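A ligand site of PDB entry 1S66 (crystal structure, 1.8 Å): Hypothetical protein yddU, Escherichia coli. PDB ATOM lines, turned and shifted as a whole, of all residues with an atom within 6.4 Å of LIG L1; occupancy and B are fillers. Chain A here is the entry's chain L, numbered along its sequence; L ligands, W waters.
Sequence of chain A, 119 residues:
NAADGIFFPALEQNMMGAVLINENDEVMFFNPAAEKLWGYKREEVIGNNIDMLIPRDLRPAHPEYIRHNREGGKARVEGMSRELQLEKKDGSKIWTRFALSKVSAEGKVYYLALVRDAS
Water W1 lies within hydrogen-bond range of O of Tyr 65, O4 of LIG L1 and ND1 of His 68.
The backbone NH of Leu 100 is in hydrogen-bond range of the backbone carbonyl oxygen of Met 80.
The backbone NH (N) of Ile 21 is in hydrogen-bond range of the backbone carbonyl oxygen (O) of Tyr 111 (3.2 Å).
The backbone NH (N) of Ala 113 is in hydrogen-bond range of the backbone carbonyl oxygen (O) of Val 19 (3.3 Å).
The backbone NH (N) of Phe 98 lies within hydrogen-bond range of the backbone carbonyl oxygen (O) of Arg 82.
The indole nitrogen (NE1) of Trp 38 sits at hydrogen-bond distance from the backbone carbonyl oxygen (O) of Leu 53 (3.1 Å).
The backbone carbonyl oxygen (O) of Leu 84 sits at hydrogen-bond distance from the side-chain hydroxyl (OG1) of Thr 96.
The side-chain amide nitrogen (ND2) of Asn 69 lies within hydrogen-bond range of the side-chain hydroxyl (OH) of Tyr 111.
FE1 of LIG L1 is bound by NE2 of His 62 (2.2 Å).
O4 of LIG L1 lies close to OD1 of Asn 69 (3.0 Å).
NE of Arg 82 is in salt-bridge range of O2 of LIG L1.
O2 of LG2 L2 is in hydrogen-bond range of NH2 of Arg 82, 3.2 Å away.
Merely in contact with LIG L1: Val 19 (3.1 Å), Tyr 111 (3.2 Å), Phe 98 (3.3 Å), Leu 58 (3.4 Å), Tyr 65 (3.4 Å), Leu 100 (3.4 Å), Ile 54 (3.4 Å), Leu 53 (3.5 Å), Pro 55 (3.5 Å), Ile 21 (3.6 Å), Ile 50 (3.7 Å), Met 80 (3.7 Å), Leu 84 (3.7 Å), Ala 113 (3.7 Å), Leu 86 (3.7 Å), Ile 66 (3.8 Å), Gln 85 (3.8 Å) and Trp 38 (3.9 Å).
21 residues have an atom within 4 Å of LIG L1: Val 19, Ile 21, Trp 38, Ile 50, Leu 53, Ile 54, Pro 55, Leu 58, His 62, Tyr 65, Ile 66, Asn 69, Met 80, Arg 82, Leu 84, Gln 85, Leu 86, Phe 98, Leu 100, Tyr 111 and Ala 113.
The nearest printed residue that does not touch LIG L1 is Leu 112 (4.4 Å).
O1 of LG2 L2 binds FE1 of LIG L1.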
ATOM      1  N   VAL A  19      13.090   2.126  15.636  1.00  0.00           N
ATOM      2  CA  VAL A  19      13.298   2.257  17.069  1.00  0.00           C
ATOM      3  C   VAL A  19      14.351   1.240  17.531  1.00  0.00           C
ATOM      4  O   VAL A  19      14.052   0.057  17.683  1.00  0.00           O
ATOM      5  CB  VAL A  19      11.983   2.033  17.854  1.00  0.00           C
ATOM      6  CG1 VAL A  19      12.186   2.266  19.342  1.00  0.00           C
ATOM      7  CG2 VAL A  19      10.875   2.923  17.305  1.00  0.00           C
ATOM      8  N   LEU A  20      15.569   1.713  17.735  1.00  0.00           N
ATOM      9  CA  LEU A  20      16.652   0.863  18.241  1.00  0.00           C
ATOM     10  C   LEU A  20      16.746   1.003  19.759  1.00  0.00           C
ATOM     11  O   LEU A  20      16.580   2.098  20.296  1.00  0.00           O
ATOM     12  CB  LEU A  20      17.988   1.251  17.600  1.00  0.00           C
ATOM     13  CG  LEU A  20      19.149   0.266  17.773  1.00  0.00           C
ATOM     14  CD1 LEU A  20      18.942  -0.986  16.938  1.00  0.00           C
ATOM     15  CD2 LEU A  20      20.465   0.938  17.392  1.00  0.00           C
ATOM     16  N   ILE A  21      16.998  -0.113  20.439  1.00  0.00           N
ATOM     17  CA  ILE A  21      17.222  -0.114  21.886  1.00  0.00           C
ATOM     18  C   ILE A  21      18.515  -0.873  22.216  1.00  0.00           C
ATOM     19  O   ILE A  21      18.847  -1.860  21.570  1.00  0.00           O
ATOM     20  CB  ILE A  21      16.016  -0.728  22.652  1.00  0.00           C
ATOM     21  CG1 ILE A  21      15.708  -2.151  22.171  1.00  0.00           C
ATOM     22  CG2 ILE A  21      14.788   0.144  22.499  1.00  0.00           C
ATOM     23  CD1 ILE A  21      14.744  -2.908  23.073  1.00  0.00           C
ATOM     24  N   TRP A  38       3.989   7.422  16.344  1.00  0.00           N
ATOM     25  CA  TRP A  38       3.741   7.451  17.785  1.00  0.00           C
ATOM     26  C   TRP A  38       3.245   8.809  18.283  1.00  0.00           C
ATOM     27  O   TRP A  38       2.594   8.889  19.327  1.00  0.00           O
ATOM     28  CB  TRP A  38       5.010   7.063  18.562  1.00  0.00           C
ATOM     29  CG  TRP A  38       5.079   5.621  18.918  1.00  0.00           C
ATOM     30  CD1 TRP A  38       4.396   4.994  19.913  1.00  0.00           C
ATOM     31  CD2 TRP A  38       5.882   4.611  18.289  1.00  0.00           C
ATOM     32  NE1 TRP A  38       4.713   3.659  19.946  1.00  0.00           N
ATOM     33  CE2 TRP A  38       5.625   3.396  18.963  1.00  0.00           C
ATOM     34  CE3 TRP A  38       6.803   4.616  17.233  1.00  0.00           C
ATOM     35  CZ2 TRP A  38       6.252   2.199  18.595  1.00  0.00           C
ATOM     36  CZ3 TRP A  38       7.415   3.423  16.878  1.00  0.00           C
ATOM     37  CH2 TRP A  38       7.140   2.229  17.554  1.00  0.00           C
ATOM     38  N   ILE A  50      11.983   1.302  27.097  1.00  0.00           N
ATOM     39  CA  ILE A  50      11.174   0.849  25.962  1.00  0.00           C
ATOM     40  C   ILE A  50       9.677   0.803  26.267  1.00  0.00           C
ATOM     41  O   ILE A  50       8.853   0.886  25.350  1.00  0.00           O
ATOM     42  CB  ILE A  50      11.670  -0.544  25.444  1.00  0.00           C
ATOM     43  CG1 ILE A  50      10.960  -0.961  24.147  1.00  0.00           C
ATOM     44  CG2 ILE A  50      11.465  -1.638  26.494  1.00  0.00           C
ATOM     45  CD1 ILE A  50      10.973   0.070  23.036  1.00  0.00           C
ATOM     46  N   LEU A  53       6.860   3.332  24.842  1.00  0.00           N
ATOM     47  CA  LEU A  53       6.345   3.131  23.483  1.00  0.00           C
ATOM     48  C   LEU A  53       5.405   1.927  23.376  1.00  0.00           C
ATOM     49  O   LEU A  53       4.811   1.699  22.323  1.00  0.00           O
ATOM     50  CB  LEU A  53       7.502   2.947  22.507  1.00  0.00           C
ATOM     51  CG  LEU A  53       8.535   4.079  22.433  1.00  0.00           C
ATOM     52  CD1 LEU A  53       9.696   3.674  21.545  1.00  0.00           C
ATOM     53  CD2 LEU A  53       7.899   5.366  21.944  1.00  0.00           C
ATOM     54  N   ILE A  54       5.268   1.152  24.450  1.00  0.00           N
ATOM     55  CA  ILE A  54       4.340   0.026  24.487  1.00  0.00           C
ATOM     56  C   ILE A  54       2.973   0.540  24.952  1.00  0.00           C
ATOM     57  O   ILE A  54       2.917   1.414  25.807  1.00  0.00           O
ATOM     58  CB  ILE A  54       4.859  -1.077  25.451  1.00  0.00           C
ATOM     59  CG1 ILE A  54       6.304  -1.487  25.105  1.00  0.00           C
ATOM     60  CG2 ILE A  54       3.951  -2.303  25.433  1.00  0.00           C
ATOM     61  CD1 ILE A  54       6.499  -2.021  23.684  1.00  0.00           C
ATOM     62  N   PRO A  55       1.882   0.022  24.382  1.00  0.00           N
ATOM     63  CA  PRO A  55       0.535   0.327  24.888  1.00  0.00           C
ATOM     64  C   PRO A  55       0.366  -0.012  26.378  1.00  0.00           C
ATOM     65  O   PRO A  55       1.074  -0.877  26.881  1.00  0.00           O
ATOM     66  CB  PRO A  55      -0.380  -0.559  24.030  1.00  0.00           C
ATOM     67  CG  PRO A  55       0.387  -0.784  22.776  1.00  0.00           C
ATOM     68  CD  PRO A  55       1.824  -0.844  23.193  1.00  0.00           C
ATOM     69  N   LEU A  58      -0.650  -3.580  27.245  1.00  0.00           N
ATOM     70  CA  LEU A  58       0.401  -4.550  26.933  1.00  0.00           C
ATOM     71  C   LEU A  58       1.672  -4.325  27.753  1.00  0.00           C
ATOM     72  O   LEU A  58       2.661  -5.052  27.573  1.00  0.00           O
ATOM     73  CB  LEU A  58       0.736  -4.500  25.427  1.00  0.00           C
ATOM     74  CG  LEU A  58       0.770  -5.791  24.584  1.00  0.00           C
ATOM     75  CD1 LEU A  58       2.063  -5.863  23.773  1.00  0.00           C
ATOM     76  CD2 LEU A  58       0.604  -7.085  25.385  1.00  0.00           C
ATOM     77  N   HIS A  62       5.006  -7.113  28.269  1.00  0.00           N
ATOM     78  CA  HIS A  62       6.113  -6.839  27.340  1.00  0.00           C
ATOM     79  C   HIS A  62       7.527  -6.951  27.917  1.00  0.00           C
ATOM     80  O   HIS A  62       8.433  -7.403  27.217  1.00  0.00           O
ATOM     81  CB  HIS A  62       5.938  -5.486  26.643  1.00  0.00           C
ATOM     82  CG  HIS A  62       6.607  -5.425  25.312  1.00  0.00           C
ATOM     83  ND1 HIS A  62       7.956  -5.199  25.169  1.00  0.00           N
ATOM     84  CD2 HIS A  62       6.116  -5.579  24.059  1.00  0.00           C
ATOM     85  CE1 HIS A  62       8.273  -5.206  23.893  1.00  0.00           C
ATOM     86  NE2 HIS A  62       7.175  -5.433  23.194  1.00  0.00           N
ATOM     87  N   TYR A  65       8.602 -10.500  27.645  1.00  0.00           N
ATOM     88  CA  TYR A  65       8.904 -10.914  26.277  1.00  0.00           C
ATOM     89  C   TYR A  65      10.354 -10.612  25.900  1.00  0.00           C
ATOM     90  O   TYR A  65      11.027 -11.432  25.266  1.00  0.00           O
ATOM     91  CB  TYR A  65       7.966 -10.248  25.265  1.00  0.00           C
ATOM     92  CG  TYR A  65       6.488 -10.545  25.424  1.00  0.00           C
ATOM     93  CD1 TYR A  65       6.044 -11.773  25.918  1.00  0.00           C
ATOM     94  CD2 TYR A  65       5.524  -9.613  25.042  1.00  0.00           C
ATOM     95  CE1 TYR A  65       4.689 -12.041  26.053  1.00  0.00           C
ATOM     96  CE2 TYR A  65       4.167  -9.873  25.171  1.00  0.00           C
ATOM     97  CZ  TYR A  65       3.759 -11.097  25.675  1.00  0.00           C
ATOM     98  OH  TYR A  65       2.416 -11.354  25.804  1.00  0.00           O
ATOM     99  N   ILE A  66      10.824  -9.420  26.266  1.00  0.00           N
ATOM    100  CA  ILE A  66      12.190  -8.990  25.939  1.00  0.00           C
ATOM    101  C   ILE A  66      13.214  -9.763  26.757  1.00  0.00           C
ATOM    102  O   ILE A  66      14.248 -10.161  26.232  1.00  0.00           O
ATOM    103  CB  ILE A  66      12.360  -7.459  26.182  1.00  0.00           C
ATOM    104  CG1 ILE A  66      11.407  -6.668  25.285  1.00  0.00           C
ATOM    105  CG2 ILE A  66      13.811  -7.037  25.924  1.00  0.00           C
ATOM    106  CD1 ILE A  66      11.547  -5.160  25.423  1.00  0.00           C
ATOM    107  N   HIS A  68      13.051 -12.783  28.067  1.00  0.00           N
ATOM    108  CA  HIS A  68      13.157 -14.169  27.629  1.00  0.00           C
ATOM    109  C   HIS A  68      14.030 -14.316  26.379  1.00  0.00           C
ATOM    110  O   HIS A  68      14.810 -15.263  26.262  1.00  0.00           O
ATOM    111  CB  HIS A  68      11.765 -14.754  27.355  1.00  0.00           C
ATOM    112  CG  HIS A  68      11.780 -16.108  26.711  1.00  0.00           C
ATOM    113  ND1 HIS A  68      11.433 -16.304  25.387  1.00  0.00           N
ATOM    114  CD2 HIS A  68      12.101 -17.318  27.206  1.00  0.00           C
ATOM    115  CE1 HIS A  68      11.539 -17.586  25.102  1.00  0.00           C
ATOM    116  NE2 HIS A  68      11.938 -18.226  26.189  1.00  0.00           N
ATOM    117  N   ASN A  69      13.890 -13.372  25.447  1.00  0.00           N
ATOM    118  CA  ASN A  69      14.654 -13.389  24.203  1.00  0.00           C
ATOM    119  C   ASN A  69      16.144 -13.092  24.415  1.00  0.00           C
ATOM    120  O   ASN A  69      16.982 -13.525  23.616  1.00  0.00           O
ATOM    121  CB  ASN A  69      14.069 -12.390  23.196  1.00  0.00           C
ATOM    122  CG  ASN A  69      14.433 -12.709  21.760  1.00  0.00           C
ATOM    123  OD1 ASN A  69      13.763 -13.504  21.106  1.00  0.00           O
ATOM    124  ND2 ASN A  69      15.495 -12.100  21.265  1.00  0.00           N
ATOM    125  N   GLY A  79      14.035 -12.494  14.544  1.00  0.00           N
ATOM    126  CA  GLY A  79      12.730 -12.410  15.182  1.00  0.00           C
ATOM    127  C   GLY A  79      11.556 -12.766  14.282  1.00  0.00           C
ATOM    128  O   GLY A  79      11.413 -13.910  13.856  1.00  0.00           O
ATOM    129  N   MET A  80      10.721 -11.767  13.995  1.00  0.00           N
ATOM    130  CA  MET A  80       9.430 -12.001  13.326  1.00  0.00           C
ATOM    131  C   MET A  80       8.837 -10.743  12.693  1.00  0.00           C
ATOM    132  O   MET A  80       9.288  -9.621  12.950  1.00  0.00           O
ATOM    133  CB  MET A  80       8.437 -12.568  14.337  1.00  0.00           C
ATOM    134  CG  MET A  80       8.175 -11.661  15.534  1.00  0.00           C
ATOM    135  SD  MET A  80       7.800 -12.560  17.057  1.00  0.00           S
ATOM    136  CE  MET A  80       6.178 -13.186  16.674  1.00  0.00           C
ATOM    137  N   ARG A  82       4.828  -9.164  11.986  1.00  0.00           N
ATOM    138  CA  ARG A  82       3.385  -9.282  12.190  1.00  0.00           C
ATOM    139  C   ARG A  82       2.727  -7.930  12.490  1.00  0.00           C
ATOM    140  O   ARG A  82       3.421  -6.928  12.704  1.00  0.00           O
ATOM    141  CB  ARG A  82       3.076 -10.280  13.324  1.00  0.00           C
ATOM    142  CG  ARG A  82       3.401  -9.798  14.734  1.00  0.00           C
ATOM    143  CD  ARG A  82       4.880  -9.567  15.000  1.00  0.00           C
ATOM    144  NE  ARG A  82       5.159  -9.399  16.426  1.00  0.00           N
ATOM    145  CZ  ARG A  82       6.245  -8.810  16.937  1.00  0.00           C
ATOM    146  NH1 ARG A  82       6.383  -8.718  18.256  1.00  0.00           N
ATOM    147  NH2 ARG A  82       7.184  -8.303  16.146  1.00  0.00           N
ATOM    148  N   LEU A  84       0.638  -5.270  14.714  1.00  0.00           N
ATOM    149  CA  LEU A  84       0.436  -4.934  16.127  1.00  0.00           C
ATOM    150  C   LEU A  84      -0.284  -3.593  16.297  1.00  0.00           C
ATOM    151  O   LEU A  84      -0.099  -2.677  15.497  1.00  0.00           O
ATOM    152  CB  LEU A  84       1.786  -4.855  16.850  1.00  0.00           C
ATOM    153  CG  LEU A  84       2.690  -6.087  16.762  1.00  0.00           C
ATOM    154  CD1 LEU A  84       4.071  -5.742  17.298  1.00  0.00           C
ATOM    155  CD2 LEU A  84       2.086  -7.248  17.533  1.00  0.00           C
ATOM    156  N   GLN A  85      -1.087  -3.481  17.360  1.00  0.00           N
ATOM    157  CA  GLN A  85      -1.821  -2.245  17.640  1.00  0.00           C
ATOM    158  C   GLN A  85      -0.954  -1.235  18.405  1.00  0.00           C
ATOM    159  O   GLN A  85      -0.742  -1.370  19.617  1.00  0.00           O
ATOM    160  CB  GLN A  85      -3.102  -2.554  18.427  1.00  0.00           C
ATOM    161  CG  GLN A  85      -4.159  -1.465  18.325  1.00  0.00           C
ATOM    162  CD  GLN A  85      -5.454  -1.832  19.022  1.00  0.00           C
ATOM    163  OE1 GLN A  85      -5.440  -2.402  20.112  1.00  0.00           O
ATOM    164  NE2 GLN A  85      -6.583  -1.517  18.382  1.00  0.00           N
ATOM    165  N   LEU A  86      -0.446  -0.254  17.674  1.00  0.00           N
ATOM    166  CA  LEU A  86       0.358   0.829  18.252  1.00  0.00           C
ATOM    167  C   LEU A  86      -0.515   1.826  19.005  1.00  0.00           C
ATOM    168  O   LEU A  86      -1.582   2.195  18.527  1.00  0.00           O
ATOM    169  CB  LEU A  86       1.122   1.548  17.135  1.00  0.00           C
ATOM    170  CG  LEU A  86       2.219   2.541  17.518  1.00  0.00           C
ATOM    171  CD1 LEU A  86       3.396   2.431  16.556  1.00  0.00           C
ATOM    172  CD2 LEU A  86       1.695   3.974  17.559  1.00  0.00           C
ATOM    173  N   GLU A  87      -0.053   2.252  20.187  1.00  0.00           N
ATOM    174  CA  GLU A  87      -0.725   3.296  20.954  1.00  0.00           C
ATOM    175  C   GLU A  87       0.096   4.581  20.947  1.00  0.00           C
ATOM    176  O   GLU A  87       1.270   4.577  21.311  1.00  0.00           O
ATOM    177  CB  GLU A  87      -0.973   2.843  22.389  1.00  0.00           C
ATOM    178  CG  GLU A  87      -1.937   3.734  23.165  1.00  0.00           C
ATOM    179  CD  GLU A  87      -2.153   3.264  24.597  1.00  0.00           C
ATOM    180  OE1 GLU A  87      -3.159   2.575  24.857  1.00  0.00           O
ATOM    181  OE2 GLU A  87      -1.309   3.593  25.455  1.00  0.00           O
ATOM    182  N   THR A  96      -0.627  -1.375  12.651  1.00  0.00           N
ATOM    183  CA  THR A  96       0.666  -1.216  11.985  1.00  0.00           C
ATOM    184  C   THR A  96       1.256  -2.561  11.528  1.00  0.00           C
ATOM    185  O   THR A  96       0.580  -3.599  11.623  1.00  0.00           O
ATOM    186  CB  THR A  96       1.662  -0.510  12.946  1.00  0.00           C
ATOM    187  OG1 THR A  96       1.711  -1.196  14.204  1.00  0.00           O
ATOM    188  CG2 THR A  96       1.177   0.896  13.301  1.00  0.00           C
ATOM    189  N   PHE A  98       4.981  -4.308  12.196  1.00  0.00           N
ATOM    190  CA  PHE A  98       6.337  -4.333  12.742  1.00  0.00           C
ATOM    191  C   PHE A  98       7.209  -5.377  12.049  1.00  0.00           C
ATOM    192  O   PHE A  98       6.708  -6.307  11.397  1.00  0.00           O
ATOM    193  CB  PHE A  98       6.300  -4.610  14.239  1.00  0.00           C
ATOM    194  CG  PHE A  98       6.076  -3.378  15.086  1.00  0.00           C
ATOM    195  CD1 PHE A  98       7.051  -2.951  15.971  1.00  0.00           C
ATOM    196  CD2 PHE A  98       4.899  -2.659  14.977  1.00  0.00           C
ATOM    197  CE1 PHE A  98       6.852  -1.813  16.751  1.00  0.00           C
ATOM    198  CE2 PHE A  98       4.693  -1.526  15.752  1.00  0.00           C
ATOM    199  CZ  PHE A  98       5.671  -1.107  16.641  1.00  0.00           C
ATOM    200  N   LEU A 100      10.583  -6.845  13.684  1.00  0.00           N
ATOM    201  CA  LEU A 100      11.609  -6.894  14.728  1.00  0.00           C
ATOM    202  C   LEU A 100      12.849  -7.674  14.295  1.00  0.00           C
ATOM    203  O   LEU A 100      12.733  -8.679  13.593  1.00  0.00           O
ATOM    204  CB  LEU A 100      11.027  -7.516  16.007  1.00  0.00           C
ATOM    205  CG  LEU A 100      11.884  -7.470  17.261  1.00  0.00           C
ATOM    206  CD1 LEU A 100      12.053  -6.041  17.752  1.00  0.00           C
ATOM    207  CD2 LEU A 100      11.260  -8.336  18.352  1.00  0.00           C
ATOM    208  N   TYR A 111      17.911  -4.262  19.520  1.00  0.00           N
ATOM    209  CA  TYR A 111      16.676  -4.622  18.798  1.00  0.00           C
ATOM    210  C   TYR A 111      16.164  -3.454  17.961  1.00  0.00           C
ATOM    211  O   TYR A 111      15.874  -2.393  18.492  1.00  0.00           O
ATOM    212  CB  TYR A 111      15.575  -5.043  19.780  1.00  0.00           C
ATOM    213  CG  TYR A 111      15.827  -6.339  20.517  1.00  0.00           C
ATOM    214  CD1 TYR A 111      16.157  -6.347  21.868  1.00  0.00           C
ATOM    215  CD2 TYR A 111      15.727  -7.567  19.856  1.00  0.00           C
ATOM    216  CE1 TYR A 111      16.376  -7.541  22.550  1.00  0.00           C
ATOM    217  CE2 TYR A 111      15.945  -8.761  20.538  1.00  0.00           C
ATOM    218  CZ  TYR A 111      16.275  -8.739  21.880  1.00  0.00           C
ATOM    219  OH  TYR A 111      16.496  -9.911  22.558  1.00  0.00           O
ATOM    220  N   LEU A 112      16.037  -3.661  16.644  1.00  0.00           N
ATOM    221  CA  LEU A 112      15.491  -2.649  15.739  1.00  0.00           C
ATOM    222  C   LEU A 112      14.115  -3.079  15.219  1.00  0.00           C
ATOM    223  O   LEU A 112      13.985  -4.111  14.557  1.00  0.00           O
ATOM    224  CB  LEU A 112      16.439  -2.437  14.556  1.00  0.00           C
ATOM    225  CG  LEU A 112      16.020  -1.371  13.530  1.00  0.00           C
ATOM    226  CD1 LEU A 112      16.102   0.021  14.135  1.00  0.00           C
ATOM    227  CD2 LEU A 112      16.849  -1.459  12.259  1.00  0.00           C
ATOM    228  N   ALA A 113      13.094  -2.273  15.523  1.00  0.00           N
ATOM    229  CA  ALA A 113      11.729  -2.539  15.072  1.00  0.00           C
ATOM    230  C   ALA A 113      11.351  -1.584  13.943  1.00  0.00           C
ATOM    231  O   ALA A 113      11.186  -0.377  14.169  1.00  0.00           O
ATOM    232  CB  ALA A 113      10.756  -2.385  16.237  1.00  0.00           C
ATOM    233  N   VAL A 115       8.674  -0.178  11.511  1.00  0.00           N
ATOM    234  CA  VAL A 115       7.211  -0.053  11.571  1.00  0.00           C
ATOM    235  C   VAL A 115       6.670   0.749  10.396  1.00  0.00           C
ATOM    236  O   VAL A 115       7.320   1.673   9.906  1.00  0.00           O
ATOM    237  CB  VAL A 115       6.783   0.650  12.876  1.00  0.00           C
ATOM    238  CG1 VAL A 115       5.281   0.482  13.121  1.00  0.00           C
ATOM    239  CG2 VAL A 115       7.582   0.130  14.071  1.00  0.00           C
HETATM  240  C1  LIG L   1       7.673  -9.182  21.631  1.00  0.00           C
HETATM  241  C2  LIG L   1       4.025  -6.015  21.042  1.00  0.00           C
HETATM  242  C3  LIG L   1       7.237  -2.450  20.264  1.00  0.00           C
HETATM  243  C4  LIG L   1      10.881  -5.482  21.333  1.00  0.00           C
HETATM  244  C5  LIG L   1       6.401  -8.648  21.533  1.00  0.00           C
HETATM  245  C6  LIG L   1       5.155  -9.373  21.656  1.00  0.00           C
HETATM  246  C7  LIG L   1       4.153  -8.506  21.499  1.00  0.00           C
HETATM  247  C8  LIG L   1       4.722  -7.190  21.257  1.00  0.00           C
HETATM  248  C9  LIG L   1       2.644  -8.848  21.557  1.00  0.00           C
HETATM  249  C10 LIG L   1       5.025 -10.891  21.933  1.00  0.00           C
HETATM  250  C11 LIG L   1       5.484 -11.704  20.729  1.00  0.00           C
HETATM  251  C12 LIG L   1       4.358 -11.871  19.746  1.00  0.00           C
HETATM  252  O1  LIG L   1       3.911 -13.033  19.537  1.00  0.00           O
HETATM  253  O2  LIG L   1       3.901 -10.851  19.172  1.00  0.00           O
HETATM  254  C13 LIG L   1       4.573  -4.767  20.814  1.00  0.00           C
HETATM  255  C14 LIG L   1       3.843  -3.526  20.665  1.00  0.00           C
HETATM  256  C15 LIG L   1       4.728  -2.541  20.452  1.00  0.00           C
HETATM  257  C16 LIG L   1       6.049  -3.122  20.451  1.00  0.00           C
HETATM  258  C17 LIG L   1       2.303  -3.370  20.750  1.00  0.00           C
HETATM  259  C18 LIG L   1       4.407  -1.040  20.240  1.00  0.00           C
HETATM  260  C19 LIG L   1       3.623  -0.668  19.231  1.00  0.00           C
HETATM  261  C20 LIG L   1       8.502  -2.963  20.440  1.00  0.00           C
HETATM  262  C21 LIG L   1       9.756  -2.278  20.186  1.00  0.00           C
HETATM  263  C22 LIG L   1      10.753  -3.121  20.484  1.00  0.00           C
HETATM  264  C23 LIG L   1      10.172  -4.362  20.936  1.00  0.00           C
HETATM  265  C24 LIG L   1       9.887  -0.823  19.666  1.00  0.00           C
HETATM  266  C25 LIG L   1      12.276  -2.848  20.385  1.00  0.00           C
HETATM  267  C26 LIG L   1      12.788  -2.215  19.332  1.00  0.00           C
HETATM  268  C27 LIG L   1      10.373  -6.769  21.480  1.00  0.00           C
HETATM  269  C28 LIG L   1      11.173  -7.947  21.705  1.00  0.00           C
HETATM  270  C29 LIG L   1      10.169  -9.104  21.803  1.00  0.00           C
HETATM  271  C30 LIG L   1       8.868  -8.498  21.619  1.00  0.00           C
HETATM  272  C31 LIG L   1      12.710  -8.038  21.828  1.00  0.00           C
HETATM  273  C32 LIG L   1      10.483 -10.603  22.039  1.00  0.00           C
HETATM  274  C33 LIG L   1      10.282 -11.382  20.738  1.00  0.00           C
HETATM  275  C34 LIG L   1       9.893 -12.803  21.047  1.00  0.00           C
HETATM  276  O3  LIG L   1       8.698 -13.157  20.833  1.00  0.00           O
HETATM  277  O4  LIG L   1      10.762 -13.583  21.504  1.00  0.00           O
HETATM  278  N1  LIG L   1       6.102  -7.316  21.290  1.00  0.00           N
HETATM  279  N2  LIG L   1       5.924  -4.482  20.670  1.00  0.00           N
HETATM  280  N3  LIG L   1       8.799  -4.237  20.896  1.00  0.00           N
HETATM  281  N4  LIG L   1       9.037  -7.131  21.432  1.00  0.00           N
HETATM  282 FE1  LIG L   1       7.477  -5.808  21.040  1.00  0.00          FE
HETATM  283  O1  LG2 L   2       7.538  -6.086  18.752  1.00  0.00           O
HETATM  284  O2  LG2 L   2       8.063  -5.721  17.906  1.00  0.00           O
HETATM  285  O   HOH W   1      10.057 -13.858  24.360  1.00  0.00           O
